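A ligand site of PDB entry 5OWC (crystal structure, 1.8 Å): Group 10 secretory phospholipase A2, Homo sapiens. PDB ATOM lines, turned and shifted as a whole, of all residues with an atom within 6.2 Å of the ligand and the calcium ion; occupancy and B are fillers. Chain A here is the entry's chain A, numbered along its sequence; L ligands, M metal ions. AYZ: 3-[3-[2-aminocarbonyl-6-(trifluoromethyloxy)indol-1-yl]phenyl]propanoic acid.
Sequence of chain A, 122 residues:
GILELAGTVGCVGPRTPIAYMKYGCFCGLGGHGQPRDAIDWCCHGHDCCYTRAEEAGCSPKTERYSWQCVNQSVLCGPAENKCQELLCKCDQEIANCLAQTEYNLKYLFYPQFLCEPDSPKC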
ATOM      1  N   ILE A   2      29.946  20.443  -9.050  1.00  0.00           N
ATOM      2  CA  ILE A   2      29.342  20.144  -7.738  1.00  0.00           C
ATOM      3  C   ILE A   2      29.195  21.436  -6.896  1.00  0.00           C
ATOM      4  O   ILE A   2      28.242  21.579  -6.149  1.00  0.00           O
ATOM      5  CB  ILE A   2      30.160  19.070  -6.973  1.00  0.00           C
ATOM      6  CG1 ILE A   2      29.865  17.654  -7.461  1.00  0.00           C
ATOM      7  CG2 ILE A   2      29.823  19.040  -5.487  1.00  0.00           C
ATOM      8  CD1 ILE A   2      28.870  17.530  -8.590  1.00  0.00           C
ATOM      9  N   LEU A   5      26.188  23.207  -8.169  1.00  0.00           N
ATOM     10  CA  LEU A   5      25.026  22.427  -7.790  1.00  0.00           C
ATOM     11  C   LEU A   5      24.575  22.736  -6.354  1.00  0.00           C
ATOM     12  O   LEU A   5      23.399  23.038  -6.100  1.00  0.00           O
ATOM     13  CB  LEU A   5      25.313  20.929  -7.956  1.00  0.00           C
ATOM     14  CG  LEU A   5      24.211  19.969  -7.488  1.00  0.00           C
ATOM     15  CD1 LEU A   5      22.865  20.262  -8.140  1.00  0.00           C
ATOM     16  CD2 LEU A   5      24.672  18.556  -7.817  1.00  0.00           C
ATOM     17  N   ALA A   6      25.528  22.656  -5.424  1.00  0.00           N
ATOM     18  CA  ALA A   6      25.252  22.980  -4.024  1.00  0.00           C
ATOM     19  C   ALA A   6      24.761  24.437  -3.882  1.00  0.00           C
ATOM     20  O   ALA A   6      23.780  24.702  -3.188  1.00  0.00           O
ATOM     21  CB  ALA A   6      26.497  22.765  -3.164  1.00  0.00           C
ATOM     22  N   VAL A   9      21.151  24.983  -5.542  1.00  0.00           N
ATOM     23  CA  VAL A   9      20.173  24.339  -4.672  1.00  0.00           C
ATOM     24  C   VAL A   9      19.968  25.160  -3.381  1.00  0.00           C
ATOM     25  O   VAL A   9      18.831  25.369  -2.953  1.00  0.00           O
ATOM     26  CB  VAL A   9      20.526  22.858  -4.419  1.00  0.00           C
ATOM     27  CG1 VAL A   9      19.634  22.242  -3.331  1.00  0.00           C
ATOM     28  CG2 VAL A   9      20.370  22.046  -5.696  1.00  0.00           C
ATOM     29  N   PRO A  17      21.955  22.170   1.120  1.00  0.00           N
ATOM     30  CA  PRO A  17      22.144  21.212   0.023  1.00  0.00           C
ATOM     31  C   PRO A  17      22.587  19.807   0.487  1.00  0.00           C
ATOM     32  O   PRO A  17      22.326  18.814  -0.203  1.00  0.00           O
ATOM     33  CB  PRO A  17      23.220  21.859  -0.861  1.00  0.00           C
ATOM     34  CG  PRO A  17      23.853  22.914  -0.023  1.00  0.00           C
ATOM     35  CD  PRO A  17      22.798  23.369   0.945  1.00  0.00           C
ATOM     36  N   ILE A  18      23.228  19.769   1.661  1.00  0.00           N
ATOM     37  CA  ILE A  18      23.570  18.538   2.408  1.00  0.00           C
ATOM     38  C   ILE A  18      22.379  17.595   2.630  1.00  0.00           C
ATOM     39  O   ILE A  18      22.559  16.386   2.703  1.00  0.00           O
ATOM     40  CB  ILE A  18      24.206  18.900   3.793  1.00  0.00           C
ATOM     41  CG1 ILE A  18      25.509  19.696   3.599  1.00  0.00           C
ATOM     42  CG2 ILE A  18      24.495  17.662   4.642  1.00  0.00           C
ATOM     43  CD1 ILE A  18      26.436  19.143   2.542  1.00  0.00           C
ATOM     44  N   ALA A  19      21.173  18.160   2.717  1.00  0.00           N
ATOM     45  CA  ALA A  19      19.946  17.375   2.858  1.00  0.00           C
ATOM     46  C   ALA A  19      19.694  16.406   1.698  1.00  0.00           C
ATOM     47  O   ALA A  19      18.882  15.479   1.836  1.00  0.00           O
ATOM     48  CB  ALA A  19      18.766  18.299   3.012  1.00  0.00           C
ATOM     49  N   TYR A  20      20.350  16.627   0.560  1.00  0.00           N
ATOM     50  CA  TYR A  20      20.214  15.754  -0.620  1.00  0.00           C
ATOM     51  C   TYR A  20      21.429  14.883  -0.952  1.00  0.00           C
ATOM     52  O   TYR A  20      21.458  14.266  -2.016  1.00  0.00           O
ATOM     53  CB  TYR A  20      19.882  16.626  -1.825  1.00  0.00           C
ATOM     54  CG  TYR A  20      18.768  17.596  -1.562  1.00  0.00           C
ATOM     55  CD1 TYR A  20      17.458  17.149  -1.420  1.00  0.00           C
ATOM     56  CD2 TYR A  20      19.015  18.965  -1.434  1.00  0.00           C
ATOM     57  CE1 TYR A  20      16.424  18.030  -1.174  1.00  0.00           C
ATOM     58  CE2 TYR A  20      17.981  19.860  -1.177  1.00  0.00           C
ATOM     59  CZ  TYR A  20      16.685  19.386  -1.058  1.00  0.00           C
ATOM     60  OH  TYR A  20      15.637  20.254  -0.832  1.00  0.00           O
ATOM     61  N   MET A  21      22.421  14.822  -0.064  1.00  0.00           N
ATOM     62  CA  MET A  21      23.661  14.090  -0.341  1.00  0.00           C
ATOM     63  C   MET A  21      23.469  12.588  -0.458  1.00  0.00           C
ATOM     64  O   MET A  21      24.126  11.928  -1.259  1.00  0.00           O
ATOM     65  CB  MET A  21      24.713  14.368   0.732  1.00  0.00           C
ATOM     66  CG  MET A  21      25.493  15.640   0.463  1.00  0.00           C
ATOM     67  SD  MET A  21      26.817  15.950   1.637  1.00  0.00           S
ATOM     68  CE  MET A  21      28.168  15.094   0.828  1.00  0.00           C
ATOM     69  N   CYS A  25      16.485   6.993  -3.366  1.00  0.00           N
ATOM     70  CA  CYS A  25      17.216   6.129  -4.281  1.00  0.00           C
ATOM     71  C   CYS A  25      18.100   6.875  -5.282  1.00  0.00           C
ATOM     72  O   CYS A  25      18.997   6.275  -5.859  1.00  0.00           O
ATOM     73  CB  CYS A  25      16.227   5.241  -5.016  1.00  0.00           C
ATOM     74  SG  CYS A  25      15.420   3.985  -3.973  1.00  0.00           S
ATOM     75  N   PHE A  26      17.862   8.180  -5.468  1.00  0.00           N
ATOM     76  CA  PHE A  26      18.552   8.944  -6.520  1.00  0.00           C
ATOM     77  C   PHE A  26      19.392  10.125  -6.085  1.00  0.00           C
ATOM     78  O   PHE A  26      20.321  10.497  -6.806  1.00  0.00           O
ATOM     79  CB  PHE A  26      17.561   9.362  -7.592  1.00  0.00           C
ATOM     80  CG  PHE A  26      17.074   8.211  -8.410  1.00  0.00           C
ATOM     81  CD1 PHE A  26      17.835   7.745  -9.476  1.00  0.00           C
ATOM     82  CD2 PHE A  26      15.906   7.547  -8.085  1.00  0.00           C
ATOM     83  CE1 PHE A  26      17.412   6.658 -10.235  1.00  0.00           C
ATOM     84  CE2 PHE A  26      15.477   6.465  -8.823  1.00  0.00           C
ATOM     85  CZ  PHE A  26      16.236   6.014  -9.898  1.00  0.00           C
ATOM     86  N   CYS A  27      19.097  10.730  -4.931  1.00  0.00           N
ATOM     87  CA  CYS A  27      19.845  11.901  -4.493  1.00  0.00           C
ATOM     88  C   CYS A  27      21.152  11.466  -3.866  1.00  0.00           C
ATOM     89  O   CYS A  27      21.158  10.873  -2.783  1.00  0.00           O
ATOM     90  CB  CYS A  27      19.045  12.760  -3.516  1.00  0.00           C
ATOM     91  SG  CYS A  27      17.400  13.250  -4.056  1.00  0.00           S
ATOM     92  N   GLY A  28      22.247  11.764  -4.557  1.00  0.00           N
ATOM     93  CA  GLY A  28      23.581  11.267  -4.225  1.00  0.00           C
ATOM     94  C   GLY A  28      24.226  10.678  -5.463  1.00  0.00           C
ATOM     95  O   GLY A  28      23.606  10.613  -6.523  1.00  0.00           O
ATOM     96  N   LEU A  29      25.458  10.223  -5.315  1.00  0.00           N
ATOM     97  CA  LEU A  29      26.220   9.661  -6.446  1.00  0.00           C
ATOM     98  C   LEU A  29      25.527   8.412  -6.991  1.00  0.00           C
ATOM     99  O   LEU A  29      25.235   7.472  -6.254  1.00  0.00           O
ATOM    100  CB  LEU A  29      27.649   9.346  -6.019  1.00  0.00           C
ATOM    101  CG  LEU A  29      28.648   8.946  -7.101  1.00  0.00           C
ATOM    102  CD1 LEU A  29      28.881  10.068  -8.117  1.00  0.00           C
ATOM    103  CD2 LEU A  29      29.969   8.553  -6.453  1.00  0.00           C
ATOM    104  N   GLY A  30      25.270   8.435  -8.302  1.00  0.00           N
ATOM    105  CA  GLY A  30      24.487   7.394  -8.973  1.00  0.00           C
ATOM    106  C   GLY A  30      23.039   7.360  -8.545  1.00  0.00           C
ATOM    107  O   GLY A  30      22.452   8.384  -8.170  1.00  0.00           O
ATOM    108  N   GLY A  31      22.448   6.189  -8.609  1.00  0.00           N
ATOM    109  CA  GLY A  31      21.060   6.018  -8.230  1.00  0.00           C
ATOM    110  C   GLY A  31      20.350   5.048  -9.131  1.00  0.00           C
ATOM    111  O   GLY A  31      20.566   5.025 -10.343  1.00  0.00           O
ATOM    112  N   CYS A  42      12.925  14.568  -8.498  1.00  0.00           N
ATOM    113  CA  CYS A  42      13.791  15.693  -8.889  1.00  0.00           C
ATOM    114  C   CYS A  42      15.208  15.206  -9.121  1.00  0.00           C
ATOM    115  O   CYS A  42      15.844  15.595 -10.089  1.00  0.00           O
ATOM    116  CB  CYS A  42      13.829  16.795  -7.824  1.00  0.00           C
ATOM    117  SG  CYS A  42      12.277  17.639  -7.458  1.00  0.00           S
ATOM    118  N   CYS A  43      15.719  14.362  -8.211  1.00  0.00           N
ATOM    119  CA  CYS A  43      17.077  13.862  -8.351  1.00  0.00           C
ATOM    120  C   CYS A  43      17.205  12.906  -9.546  1.00  0.00           C
ATOM    121  O   CYS A  43      18.211  12.933 -10.247  1.00  0.00           O
ATOM    122  CB  CYS A  43      17.546  13.202  -7.060  1.00  0.00           C
ATOM    123  SG  CYS A  43      17.763  14.381  -5.718  1.00  0.00           S
ATOM    124  N   HIS A  44      16.176  12.091  -9.785  1.00  0.00           N
ATOM    125  CA  HIS A  44      16.182  11.223 -10.961  1.00  0.00           C
ATOM    126  C   HIS A  44      16.287  12.071 -12.236  1.00  0.00           C
ATOM    127  O   HIS A  44      17.106  11.781 -13.115  1.00  0.00           O
ATOM    128  CB  HIS A  44      14.923  10.361 -10.992  1.00  0.00           C
ATOM    129  CG  HIS A  44      14.781   9.564 -12.258  1.00  0.00           C
ATOM    130  ND1 HIS A  44      14.071  10.020 -13.339  1.00  0.00           N
ATOM    131  CD2 HIS A  44      15.263   8.351 -12.609  1.00  0.00           C
ATOM    132  CE1 HIS A  44      14.122   9.122 -14.308  1.00  0.00           C
ATOM    133  NE2 HIS A  44      14.846   8.098 -13.897  1.00  0.00           N
ATOM    134  N   HIS A  46      17.451  15.079 -12.545  1.00  0.00           N
ATOM    135  CA  HIS A  46      18.768  15.683 -12.559  1.00  0.00           C
ATOM    136  C   HIS A  46      19.875  14.708 -13.003  1.00  0.00           C
ATOM    137  O   HIS A  46      20.745  15.067 -13.792  1.00  0.00           O
ATOM    138  CB  HIS A  46      19.063  16.281 -11.178  1.00  0.00           C
ATOM    139  CG  HIS A  46      20.257  17.177 -11.153  1.00  0.00           C
ATOM    140  ND1 HIS A  46      21.393  16.873 -10.442  1.00  0.00           N
ATOM    141  CD2 HIS A  46      20.483  18.369 -11.744  1.00  0.00           C
ATOM    142  CE1 HIS A  46      22.274  17.845 -10.590  1.00  0.00           C
ATOM    143  NE2 HIS A  46      21.750  18.768 -11.385  1.00  0.00           N
ATOM    144  N   ASP A  47      19.832  13.469 -12.501  1.00  0.00           N
ATOM    145  CA  ASP A  47      20.736  12.411 -12.971  1.00  0.00           C
ATOM    146  C   ASP A  47      20.648  12.223 -14.490  1.00  0.00           C
ATOM    147  O   ASP A  47      21.673  12.107 -15.169  1.00  0.00           O
ATOM    148  CB  ASP A  47      20.420  11.070 -12.293  1.00  0.00           C
ATOM    149  CG  ASP A  47      20.803  11.050 -10.827  1.00  0.00           C
ATOM    150  OD1 ASP A  47      21.243  12.070 -10.243  1.00  0.00           O
ATOM    151  OD2 ASP A  47      20.674   9.959 -10.214  1.00  0.00           O
ATOM    152  N   TYR A  50      22.321  15.292 -16.210  1.00  0.00           N
ATOM    153  CA  TYR A  50      23.780  15.105 -16.198  1.00  0.00           C
ATOM    154  C   TYR A  50      24.254  14.031 -17.182  1.00  0.00           C
ATOM    155  O   TYR A  50      25.298  14.212 -17.837  1.00  0.00           O
ATOM    156  CB  TYR A  50      24.271  14.781 -14.781  1.00  0.00           C
ATOM    157  CG  TYR A  50      24.567  15.999 -13.901  1.00  0.00           C
ATOM    158  CD1 TYR A  50      23.997  17.261 -14.146  1.00  0.00           C
ATOM    159  CD2 TYR A  50      25.428  15.880 -12.810  1.00  0.00           C
ATOM    160  CE1 TYR A  50      24.294  18.356 -13.343  1.00  0.00           C
ATOM    161  CE2 TYR A  50      25.720  16.967 -11.986  1.00  0.00           C
ATOM    162  CZ  TYR A  50      25.149  18.202 -12.263  1.00  0.00           C
ATOM    163  OH  TYR A  50      25.433  19.282 -11.439  1.00  0.00           O
ATOM    164  N   LYS A  61      30.253  17.234 -13.170  1.00  0.00           N
ATOM    165  CA  LYS A  61      30.765  17.273 -11.796  1.00  0.00           C
ATOM    166  C   LYS A  61      31.843  18.316 -11.537  1.00  0.00           C
ATOM    167  O   LYS A  61      31.998  18.774 -10.409  1.00  0.00           O
ATOM    168  CB  LYS A  61      31.248  15.886 -11.363  1.00  0.00           C
ATOM    169  CG  LYS A  61      30.150  14.832 -11.410  1.00  0.00           C
ATOM    170  CD  LYS A  61      30.521  13.533 -10.698  1.00  0.00           C
ATOM    171  CE  LYS A  61      31.158  12.511 -11.636  1.00  0.00           C
ATOM    172  NZ  LYS A  61      31.541  11.255 -10.923  1.00  0.00           N
ATOM    173  N   ILE A  94      16.900  21.423 -11.167  1.00  0.00           N
ATOM    174  CA  ILE A  94      16.791  20.662  -9.917  1.00  0.00           C
ATOM    175  C   ILE A  94      16.564  21.600  -8.729  1.00  0.00           C
ATOM    176  O   ILE A  94      15.767  21.281  -7.851  1.00  0.00           O
ATOM    177  CB  ILE A  94      17.942  19.666  -9.643  1.00  0.00           C
ATOM    178  CG1 ILE A  94      17.445  18.585  -8.644  1.00  0.00           C
ATOM    179  CG2 ILE A  94      19.229  20.374  -9.219  1.00  0.00           C
ATOM    180  CD1 ILE A  94      18.513  17.744  -7.977  1.00  0.00           C
ATOM    181  N   LEU A  98      13.370  21.053  -6.322  1.00  0.00           N
ATOM    182  CA  LEU A  98      13.508  20.744  -4.890  1.00  0.00           C
ATOM    183  C   LEU A  98      12.876  21.789  -3.981  1.00  0.00           C
ATOM    184  O   LEU A  98      12.362  21.463  -2.924  1.00  0.00           O
ATOM    185  CB  LEU A  98      14.973  20.561  -4.527  1.00  0.00           C
ATOM    186  CG  LEU A  98      15.655  19.356  -5.186  1.00  0.00           C
ATOM    187  CD1 LEU A  98      17.162  19.437  -4.963  1.00  0.00           C
ATOM    188  CD2 LEU A  98      15.113  18.037  -4.658  1.00  0.00           C
HETATM  189  C1  AYZ L   1      21.326  18.184  -4.623  1.00  0.00           C
HETATM  190  C2  AYZ L   1      22.211  18.853  -3.834  1.00  0.00           C
HETATM  191  C3  AYZ L   1      23.534  18.409  -3.720  1.00  0.00           C
HETATM  192  C8  AYZ L   1      21.937  15.254  -6.657  1.00  0.00           C
HETATM  193  C9  AYZ L   1      21.043  16.180  -6.224  1.00  0.00           C
HETATM  194  C10 AYZ L   1      21.635  14.150  -7.581  1.00  0.00           C
HETATM  195  C13 AYZ L   1      24.348  14.748  -6.289  1.00  0.00           C
HETATM  196  C15 AYZ L   1      25.453  18.584  -2.296  1.00  0.00           C
HETATM  197  C19 AYZ L   1      25.191  14.223  -5.307  1.00  0.00           C
HETATM  198  C20 AYZ L   1      26.347  13.544  -5.678  1.00  0.00           C
HETATM  199  C21 AYZ L   1      26.682  13.396  -7.022  1.00  0.00           C
HETATM  200  C22 AYZ L   1      25.847  13.915  -8.014  1.00  0.00           C
HETATM  201  C24 AYZ L   1      26.177  13.774  -9.477  1.00  0.00           C
HETATM  202  O28 AYZ L   1      26.064  10.915 -10.035  1.00  0.00           O
HETATM  203  C4  AYZ L   1      23.971  17.283  -4.424  1.00  0.00           C
HETATM  204  C5  AYZ L   1      21.734  17.043  -5.337  1.00  0.00           C
HETATM  205  C6  AYZ L   1      23.064  16.580  -5.244  1.00  0.00           C
HETATM  206  N7  AYZ L   1      23.165  15.468  -6.034  1.00  0.00           N
HETATM  207  N11 AYZ L   1      20.958  14.413  -8.723  1.00  0.00           N
HETATM  208  O12 AYZ L   1      21.991  12.994  -7.312  1.00  0.00           O
HETATM  209  O14 AYZ L   1      24.345  19.161  -2.934  1.00  0.00           O
HETATM  210  F16 AYZ L   1      24.951  17.471  -1.629  1.00  0.00           F
HETATM  211  F17 AYZ L   1      26.425  18.261  -3.253  1.00  0.00           F
HETATM  212  F18 AYZ L   1      25.953  19.488  -1.360  1.00  0.00           F
HETATM  213  C23 AYZ L   1      24.704  14.609  -7.633  1.00  0.00           C
HETATM  214  C25 AYZ L   1      25.073  13.062 -10.279  1.00  0.00           C
HETATM  215  C26 AYZ L   1      25.052  11.573  -9.981  1.00  0.00           C
HETATM  216  O27 AYZ L   1      23.918  10.946  -9.666  1.00  0.00           O
HETATM  217 CA    CA M   1      22.054  10.728  -8.278  1.00  0.00          CA
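A nitrogen (N11) of the ligand lies within hydrogen-bond range of a ring nitrogen (ND1) of His 46, 3.0 Å away. A nitrogen (N11) of the ligand is in hydrogen-bond range of the backbone carbonyl oxygen (O) of Cys 43, at 3.5 Å. An oxygen (O12) of the ligand lies close to the backbone NH of Gly 28 (3.0 Å). An oxygen (O28) of the ligand lies within hydrogen-bond range of the backbone NH (N) of Gly 30 (3.1 Å).
The side-chain sulfur (SG) of Cys 43 is disulfide-bonded to the side-chain sulfur (SG) of Cys 27 (2.0 Å).
A fluorine (F16) of the ligand lies close to the backbone carbonyl oxygen (O) of Pro 17 (3.3 Å). CD2 of Leu 5 touches C6 of the ligand, at 3.6 Å. CB of Ala 6 touches F18 of the ligand, at 3.8 Å. Ile 18 touches the ligand. Tyr 20 touches the ligand (CB to C1, 3.5 Å). Met 21 touches the ligand. Cys 27 touches the ligand (CA to O12, 3.7 Å). N of Leu 29 touches C20 of the ligand (3.5 Å). Tyr 50 touches the ligand (CD2 to C25, 3.8 Å). Ile 94 touches the ligand. Hydrophobic or aromatic side chains that line the ligand: Leu 5, Ala 6, Pro 17, Ile 18, Tyr 20, Met 21, Leu 29, His 46, Tyr 50 and Ile 94. Of the 25 residues printed, 16 come within 4 Å of the ligand.
Within 4 Å of the calcium ion: Phe 26, Gly 28, Gly 30 and Asp 47.
The backbone carbonyl oxygen (O) of Phe 26 is bound to the calcium ion (2.3 Å). The calcium ion is bound by O27 of the ligand, at 2.3 Å. The backbone carbonyl oxygen (O) of Gly 28 is bound to the calcium ion (2.3 Å). O of Gly 30 binds the calcium ion (2.4 Å). O12 of the ligand is bound to the calcium ion (2.5 Å). The side-chain carboxylate (OD2) of Asp 47 binds the calcium ion. OD1 of Asp 47 is bound to the calcium ion (2.5 Å). The calcium ion has seven donor atoms within binding distance.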
